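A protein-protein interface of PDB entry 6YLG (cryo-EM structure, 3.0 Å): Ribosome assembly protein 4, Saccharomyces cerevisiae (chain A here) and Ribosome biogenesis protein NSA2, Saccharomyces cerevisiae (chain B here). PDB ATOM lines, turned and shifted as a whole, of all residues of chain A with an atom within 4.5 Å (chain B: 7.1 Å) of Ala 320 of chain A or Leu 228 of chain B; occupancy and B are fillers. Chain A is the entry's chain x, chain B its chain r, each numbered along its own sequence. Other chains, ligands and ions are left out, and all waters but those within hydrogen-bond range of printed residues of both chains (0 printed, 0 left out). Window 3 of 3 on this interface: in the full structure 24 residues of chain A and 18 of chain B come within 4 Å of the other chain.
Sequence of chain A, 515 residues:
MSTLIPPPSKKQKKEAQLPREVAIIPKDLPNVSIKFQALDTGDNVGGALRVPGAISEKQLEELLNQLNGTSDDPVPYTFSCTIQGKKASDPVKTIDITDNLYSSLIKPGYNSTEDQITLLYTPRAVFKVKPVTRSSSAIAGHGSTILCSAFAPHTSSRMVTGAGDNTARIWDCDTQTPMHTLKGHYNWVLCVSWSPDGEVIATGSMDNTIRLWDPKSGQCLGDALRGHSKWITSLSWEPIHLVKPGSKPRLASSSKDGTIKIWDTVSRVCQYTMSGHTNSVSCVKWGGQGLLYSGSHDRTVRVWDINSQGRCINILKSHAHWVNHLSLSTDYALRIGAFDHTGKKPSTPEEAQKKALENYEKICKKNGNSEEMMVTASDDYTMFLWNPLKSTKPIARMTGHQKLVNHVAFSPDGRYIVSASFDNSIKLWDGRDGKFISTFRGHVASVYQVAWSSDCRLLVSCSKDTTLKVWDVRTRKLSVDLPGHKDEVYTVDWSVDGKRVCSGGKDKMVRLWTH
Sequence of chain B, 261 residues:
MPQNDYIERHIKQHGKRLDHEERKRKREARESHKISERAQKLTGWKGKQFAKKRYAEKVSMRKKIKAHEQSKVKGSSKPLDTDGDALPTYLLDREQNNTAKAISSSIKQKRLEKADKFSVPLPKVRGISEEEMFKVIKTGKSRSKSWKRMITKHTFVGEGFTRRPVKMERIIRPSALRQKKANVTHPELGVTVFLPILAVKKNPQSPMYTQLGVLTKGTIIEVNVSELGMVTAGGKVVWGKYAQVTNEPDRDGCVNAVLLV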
ATOM      1  N   ARG A 299      -3.777  29.453  -3.204  1.00  0.00           N
ATOM      2  CA  ARG A 299      -3.142  28.174  -2.892  1.00  0.00           C
ATOM      3  C   ARG A 299      -3.488  27.673  -1.497  1.00  0.00           C
ATOM      4  O   ARG A 299      -2.743  26.866  -0.931  1.00  0.00           O
ATOM      5  CB  ARG A 299      -1.618  28.249  -3.039  1.00  0.00           C
ATOM      6  CG  ARG A 299      -1.120  28.875  -4.328  1.00  0.00           C
ATOM      7  CD  ARG A 299       0.364  29.120  -4.240  1.00  0.00           C
ATOM      8  NE  ARG A 299       0.660  30.285  -3.411  1.00  0.00           N
ATOM      9  CZ  ARG A 299       1.832  30.536  -2.831  1.00  0.00           C
ATOM     10  NH1 ARG A 299       2.863  29.706  -2.966  1.00  0.00           N
ATOM     11  NH2 ARG A 299       1.971  31.632  -2.102  1.00  0.00           N
ATOM     12  N   SER A 318      -1.042  23.357   1.248  1.00  0.00           N
ATOM     13  CA  SER A 318      -0.132  22.365   0.680  1.00  0.00           C
ATOM     14  C   SER A 318       0.093  22.509  -0.816  1.00  0.00           C
ATOM     15  O   SER A 318       1.112  22.015  -1.308  1.00  0.00           O
ATOM     16  CB  SER A 318      -0.642  20.952   0.969  1.00  0.00           C
ATOM     17  OG  SER A 318      -0.744  20.731   2.363  1.00  0.00           O
ATOM     18  N   HIS A 319      -0.799  23.159  -1.558  1.00  0.00           N
ATOM     19  CA  HIS A 319      -0.650  23.270  -2.998  1.00  0.00           C
ATOM     20  C   HIS A 319       0.390  24.326  -3.359  1.00  0.00           C
ATOM     21  O   HIS A 319       0.714  25.219  -2.572  1.00  0.00           O
ATOM     22  CB  HIS A 319      -1.983  23.622  -3.652  1.00  0.00           C
ATOM     23  CG  HIS A 319      -2.862  22.439  -3.910  1.00  0.00           C
ATOM     24  ND1 HIS A 319      -2.654  21.574  -4.962  1.00  0.00           N
ATOM     25  CD2 HIS A 319      -3.954  21.980  -3.256  1.00  0.00           C
ATOM     26  CE1 HIS A 319      -3.583  20.635  -4.948  1.00  0.00           C
ATOM     27  NE2 HIS A 319      -4.382  20.856  -3.920  1.00  0.00           N
ATOM     28  N   ALA A 320       0.909  24.207  -4.582  1.00  0.00           N
ATOM     29  CA  ALA A 320       1.902  25.127  -5.123  1.00  0.00           C
ATOM     30  C   ALA A 320       1.304  26.092  -6.136  1.00  0.00           C
ATOM     31  O   ALA A 320       1.761  27.234  -6.245  1.00  0.00           O
ATOM     32  CB  ALA A 320       3.037  24.343  -5.779  1.00  0.00           C
ATOM     33  N   HIS A 321       0.292  25.650  -6.876  1.00  0.00           N
ATOM     34  CA  HIS A 321      -0.414  26.456  -7.861  1.00  0.00           C
ATOM     35  C   HIS A 321      -1.854  26.629  -7.386  1.00  0.00           C
ATOM     36  O   HIS A 321      -2.208  26.254  -6.266  1.00  0.00           O
ATOM     37  CB  HIS A 321      -0.333  25.818  -9.247  1.00  0.00           C
ATOM     38  CG  HIS A 321      -0.067  26.796 -10.352  1.00  0.00           C
ATOM     39  ND1 HIS A 321      -0.886  27.872 -10.612  1.00  0.00           N
ATOM     40  CD2 HIS A 321       0.927  26.852 -11.271  1.00  0.00           C
ATOM     41  CE1 HIS A 321      -0.409  28.551 -11.638  1.00  0.00           C
ATOM     42  NE2 HIS A 321       0.690  27.953 -12.057  1.00  0.00           N
ATOM     43  N   ASP A 380      -0.933  22.642 -10.174  1.00  0.00           N
ATOM     44  CA  ASP A 380       0.342  21.961 -10.009  1.00  0.00           C
ATOM     45  C   ASP A 380       0.264  20.490 -10.401  1.00  0.00           C
ATOM     46  O   ASP A 380       1.145  19.712 -10.020  1.00  0.00           O
ATOM     47  CB  ASP A 380       0.828  22.096  -8.564  1.00  0.00           C
ATOM     48  CG  ASP A 380       0.024  21.265  -7.597  1.00  0.00           C
ATOM     49  OD1 ASP A 380      -1.177  21.052  -7.860  1.00  0.00           O
ATOM     50  OD2 ASP A 380       0.588  20.822  -6.575  1.00  0.00           O
ATOM     51  N   HIS B 186       6.154  34.873  -9.709  1.00  0.00           N
ATOM     52  CA  HIS B 186       5.359  34.010 -10.543  1.00  0.00           C
ATOM     53  C   HIS B 186       4.327  34.871 -11.255  1.00  0.00           C
ATOM     54  O   HIS B 186       3.613  35.618 -10.571  1.00  0.00           O
ATOM     55  CB  HIS B 186       4.672  32.952  -9.684  1.00  0.00           C
ATOM     56  CG  HIS B 186       4.324  31.700 -10.423  1.00  0.00           C
ATOM     57  ND1 HIS B 186       3.585  31.701 -11.585  1.00  0.00           N
ATOM     58  CD2 HIS B 186       4.607  30.404 -10.157  1.00  0.00           C
ATOM     59  CE1 HIS B 186       3.431  30.458 -12.005  1.00  0.00           C
ATOM     60  NE2 HIS B 186       4.042  29.652 -11.157  1.00  0.00           N
ATOM     61  N   LEU B 189      -0.617  33.732  -9.949  1.00  0.00           N
ATOM     62  CA  LEU B 189      -0.699  33.814  -8.490  1.00  0.00           C
ATOM     63  C   LEU B 189      -0.448  35.212  -7.932  1.00  0.00           C
ATOM     64  O   LEU B 189      -0.702  35.444  -6.745  1.00  0.00           O
ATOM     65  CB  LEU B 189       0.286  32.849  -7.816  1.00  0.00           C
ATOM     66  CG  LEU B 189       0.394  31.406  -8.306  1.00  0.00           C
ATOM     67  CD1 LEU B 189       1.708  30.795  -7.847  1.00  0.00           C
ATOM     68  CD2 LEU B 189      -0.778  30.601  -7.794  1.00  0.00           C
ATOM     69  N   VAL B 191       2.198  36.692  -7.022  1.00  0.00           N
ATOM     70  CA  VAL B 191       2.964  36.456  -5.802  1.00  0.00           C
ATOM     71  C   VAL B 191       4.446  36.553  -6.127  1.00  0.00           C
ATOM     72  O   VAL B 191       4.877  36.167  -7.219  1.00  0.00           O
ATOM     73  CB  VAL B 191       2.613  35.085  -5.186  1.00  0.00           C
ATOM     74  CG1 VAL B 191       3.718  34.545  -4.274  1.00  0.00           C
ATOM     75  CG2 VAL B 191       1.318  35.190  -4.411  1.00  0.00           C
ATOM     76  N   THR B 192       5.217  37.076  -5.179  1.00  0.00           N
ATOM     77  CA  THR B 192       6.664  37.143  -5.257  1.00  0.00           C
ATOM     78  C   THR B 192       7.286  36.480  -4.037  1.00  0.00           C
ATOM     79  O   THR B 192       6.657  36.331  -2.988  1.00  0.00           O
ATOM     80  CB  THR B 192       7.127  38.591  -5.350  1.00  0.00           C
ATOM     81  OG1 THR B 192       6.700  39.299  -4.182  1.00  0.00           O
ATOM     82  CG2 THR B 192       6.532  39.241  -6.558  1.00  0.00           C
ATOM     83  N   VAL B 193       8.545  36.084  -4.191  1.00  0.00           N
ATOM     84  CA  VAL B 193       9.275  35.367  -3.158  1.00  0.00           C
ATOM     85  C   VAL B 193      10.748  35.732  -3.235  1.00  0.00           C
ATOM     86  O   VAL B 193      11.299  35.963  -4.315  1.00  0.00           O
ATOM     87  CB  VAL B 193       9.086  33.840  -3.278  1.00  0.00           C
ATOM     88  CG1 VAL B 193       7.735  33.431  -2.739  1.00  0.00           C
ATOM     89  CG2 VAL B 193       9.213  33.406  -4.728  1.00  0.00           C
ATOM     90  N   LEU B 195      13.955  34.303  -3.126  1.00  0.00           N
ATOM     91  CA  LEU B 195      14.500  32.964  -3.314  1.00  0.00           C
ATOM     92  C   LEU B 195      16.018  33.005  -3.447  1.00  0.00           C
ATOM     93  O   LEU B 195      16.560  34.008  -3.918  1.00  0.00           O
ATOM     94  CB  LEU B 195      13.923  32.298  -4.566  1.00  0.00           C
ATOM     95  CG  LEU B 195      12.411  32.112  -4.652  1.00  0.00           C
ATOM     96  CD1 LEU B 195      12.036  31.681  -6.053  1.00  0.00           C
ATOM     97  CD2 LEU B 195      11.936  31.098  -3.638  1.00  0.00           C
ATOM     98  N   ASN B 224      16.214  28.353  -6.651  1.00  0.00           N
ATOM     99  CA  ASN B 224      15.580  27.277  -5.901  1.00  0.00           C
ATOM    100  C   ASN B 224      14.105  27.602  -5.711  1.00  0.00           C
ATOM    101  O   ASN B 224      13.743  28.766  -5.510  1.00  0.00           O
ATOM    102  CB  ASN B 224      16.273  27.092  -4.555  1.00  0.00           C
ATOM    103  CG  ASN B 224      15.786  25.870  -3.805  1.00  0.00           C
ATOM    104  OD1 ASN B 224      14.850  25.192  -4.226  1.00  0.00           O
ATOM    105  ND2 ASN B 224      16.418  25.588  -2.676  1.00  0.00           N
ATOM    106  N   VAL B 225      13.264  26.572  -5.770  1.00  0.00           N
ATOM    107  CA  VAL B 225      11.817  26.711  -5.682  1.00  0.00           C
ATOM    108  C   VAL B 225      11.217  25.738  -4.672  1.00  0.00           C
ATOM    109  O   VAL B 225      10.010  25.479  -4.707  1.00  0.00           O
ATOM    110  CB  VAL B 225      11.166  26.545  -7.065  1.00  0.00           C
ATOM    111  CG1 VAL B 225      11.352  27.805  -7.879  1.00  0.00           C
ATOM    112  CG2 VAL B 225      11.760  25.368  -7.795  1.00  0.00           C
ATOM    113  N   SER B 226      12.031  25.194  -3.764  1.00  0.00           N
ATOM    114  CA  SER B 226      11.528  24.259  -2.767  1.00  0.00           C
ATOM    115  C   SER B 226      10.523  24.897  -1.818  1.00  0.00           C
ATOM    116  O   SER B 226       9.711  24.180  -1.225  1.00  0.00           O
ATOM    117  CB  SER B 226      12.693  23.679  -1.970  1.00  0.00           C
ATOM    118  OG  SER B 226      13.543  24.708  -1.500  1.00  0.00           O
ATOM    119  N   GLU B 227      10.557  26.222  -1.660  1.00  0.00           N
ATOM    120  CA  GLU B 227       9.596  26.886  -0.786  1.00  0.00           C
ATOM    121  C   GLU B 227       8.179  26.799  -1.336  1.00  0.00           C
ATOM    122  O   GLU B 227       7.212  26.936  -0.579  1.00  0.00           O
ATOM    123  CB  GLU B 227       9.989  28.349  -0.597  1.00  0.00           C
ATOM    124  CG  GLU B 227      11.385  28.556  -0.047  1.00  0.00           C
ATOM    125  CD  GLU B 227      11.708  30.019   0.184  1.00  0.00           C
ATOM    126  OE1 GLU B 227      12.547  30.316   1.061  1.00  0.00           O
ATOM    127  OE2 GLU B 227      11.119  30.873  -0.508  1.00  0.00           O
ATOM    128  N   LEU B 228       8.036  26.564  -2.643  1.00  0.00           N
ATOM    129  CA  LEU B 228       6.720  26.591  -3.269  1.00  0.00           C
ATOM    130  C   LEU B 228       6.068  25.214  -3.260  1.00  0.00           C
ATOM    131  O   LEU B 228       4.856  25.096  -3.473  1.00  0.00           O
ATOM    132  CB  LEU B 228       6.845  27.118  -4.696  1.00  0.00           C
ATOM    133  CG  LEU B 228       7.376  28.552  -4.813  1.00  0.00           C
ATOM    134  CD1 LEU B 228       7.668  28.924  -6.255  1.00  0.00           C
ATOM    135  CD2 LEU B 228       6.402  29.550  -4.199  1.00  0.00           C
ATOM    136  N   GLY B 229       6.845  24.163  -3.016  1.00  0.00           N
ATOM    137  CA  GLY B 229       6.288  22.831  -2.912  1.00  0.00           C
ATOM    138  C   GLY B 229       5.875  22.256  -4.249  1.00  0.00           C
ATOM    139  O   GLY B 229       4.907  21.496  -4.333  1.00  0.00           O
ATOM    140  N   MET B 230       6.606  22.609  -5.301  1.00  0.00           N
ATOM    141  CA  MET B 230       6.310  22.093  -6.626  1.00  0.00           C
ATOM    142  C   MET B 230       6.805  20.660  -6.747  1.00  0.00           C
ATOM    143  O   MET B 230       7.845  20.295  -6.189  1.00  0.00           O
ATOM    144  CB  MET B 230       6.957  22.967  -7.697  1.00  0.00           C
ATOM    145  CG  MET B 230       6.292  24.310  -7.853  1.00  0.00           C
ATOM    146  SD  MET B 230       7.457  25.648  -8.136  1.00  0.00           S
ATOM    147  CE  MET B 230       7.491  25.646  -9.921  1.00  0.00           C
ATOM    148  N   VAL B 231       6.049  19.849  -7.477  1.00  0.00           N
ATOM    149  CA  VAL B 231       6.319  18.425  -7.615  1.00  0.00           C
ATOM    150  C   VAL B 231       5.903  18.003  -9.015  1.00  0.00           C
ATOM    151  O   VAL B 231       4.871  18.458  -9.522  1.00  0.00           O
ATOM    152  CB  VAL B 231       5.583  17.592  -6.549  1.00  0.00           C
ATOM    153  CG1 VAL B 231       4.079  17.847  -6.583  1.00  0.00           C
ATOM    154  CG2 VAL B 231       5.865  16.119  -6.734  1.00  0.00           C
ATOM    155  N   VAL B 238      10.526  19.357  -7.184  1.00  0.00           N
ATOM    156  CA  VAL B 238      11.320  20.276  -7.985  1.00  0.00           C
ATOM    157  C   VAL B 238      11.961  21.280  -7.041  1.00  0.00           C
ATOM    158  O   VAL B 238      11.295  21.819  -6.151  1.00  0.00           O
ATOM    159  CB  VAL B 238      10.468  20.996  -9.048  1.00  0.00           C
ATOM    160  CG1 VAL B 238      11.302  22.025  -9.779  1.00  0.00           C
ATOM    161  CG2 VAL B 238       9.878  19.996 -10.020  1.00  0.00           C
ATOM    162  N   LEU B 259       9.697  34.218 -13.065  1.00  0.00           N
ATOM    163  CA  LEU B 259       9.861  32.791 -13.298  1.00  0.00           C
ATOM    164  C   LEU B 259       9.484  32.444 -14.730  1.00  0.00           C
ATOM    165  O   LEU B 259       8.571  33.041 -15.307  1.00  0.00           O
ATOM    166  CB  LEU B 259       8.985  31.980 -12.340  1.00  0.00           C
ATOM    167  CG  LEU B 259       9.583  31.141 -11.214  1.00  0.00           C
ATOM    168  CD1 LEU B 259       8.490  30.254 -10.664  1.00  0.00           C
ATOM    169  CD2 LEU B 259      10.749  30.294 -11.674  1.00  0.00           C
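The backbone NH (N) of His 186 of chain B sits at hydrogen-bond distance from the backbone carbonyl oxygen (O) of Val 191 of chain B (3.1 Å).
O of Met 230 of chain B is in hydrogen-bond range of N of Val 238 of chain B (3.0 Å).
OD1 of Asp 380 of chain A sits at hydrogen-bond distance from ND1 of His 319 of chain A (3.3 Å).
Arg 299 of chain A touches Leu 189 of chain B (CG to CD2, 3.9 Å).
Arg 299 of chain A touches Leu 228 of chain B (NH1 to CD2, 3.8 Å).
CD1 of Leu 189 of chain B touches O of Ala 320 of chain A, at 3.9 Å.
Leu 228 of chain B touches Ala 320 of chain A (O to CB, 3.0 Å).
O of Gly 229 of chain B touches CB of Ala 320 of chain A (3.7 Å).
Met 230 of chain B touches Ala 320 of chain A (CG to CB, 3.9 Å).
His 321 of chain A touches His 186 of chain B.
Leu 189 of chain B touches His 321 of chain A (CD2 to ND1, 3.9 Å).
O of Asp 380 of chain A touches O of Val 231 of chain B, at 3.96 Å.
Printed residues of chain B that touch a printed residue of chain A: His 186, Leu 189, Leu 228, Gly 229, Met 230 and Val 231.
Hydrophobic or aromatic side chains of chain B that line the printed part of chain A: His 186, Leu 189, Leu 228 and Met 230.
Of the printed residues of chain B, Ala 320 of chain A touches Leu 189 (3.9 Å), Leu 228 (3.0 Å), Gly 229 (3.7 Å) and Met 230 (3.9 Å).
Leu 228 of chain B touches just these residues of chain A: Arg 299 (3.8 Å) and Ala 320 (3.0 Å).
Printed residues of chain B within 4 Å of Arg 299 of chain A: Leu 189 and Leu 228.
Of the printed residues of chain A, His 186 of chain B touches His 321 (3.7 Å).
Of the printed residues of chain B, His 321 of chain A touches His 186 (3.7 Å) and Leu 189 (3.9 Å).
Of the printed residues of chain A, Met 230 of chain B touches Ala 320.
Printed residues of chain B within 4 Å of Asp 380 of chain A: Val 231 (3.96 Å).
The nearest residue of chain A that does not touch Leu 228 of chain B is His 319 of chain A (4.2 Å).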
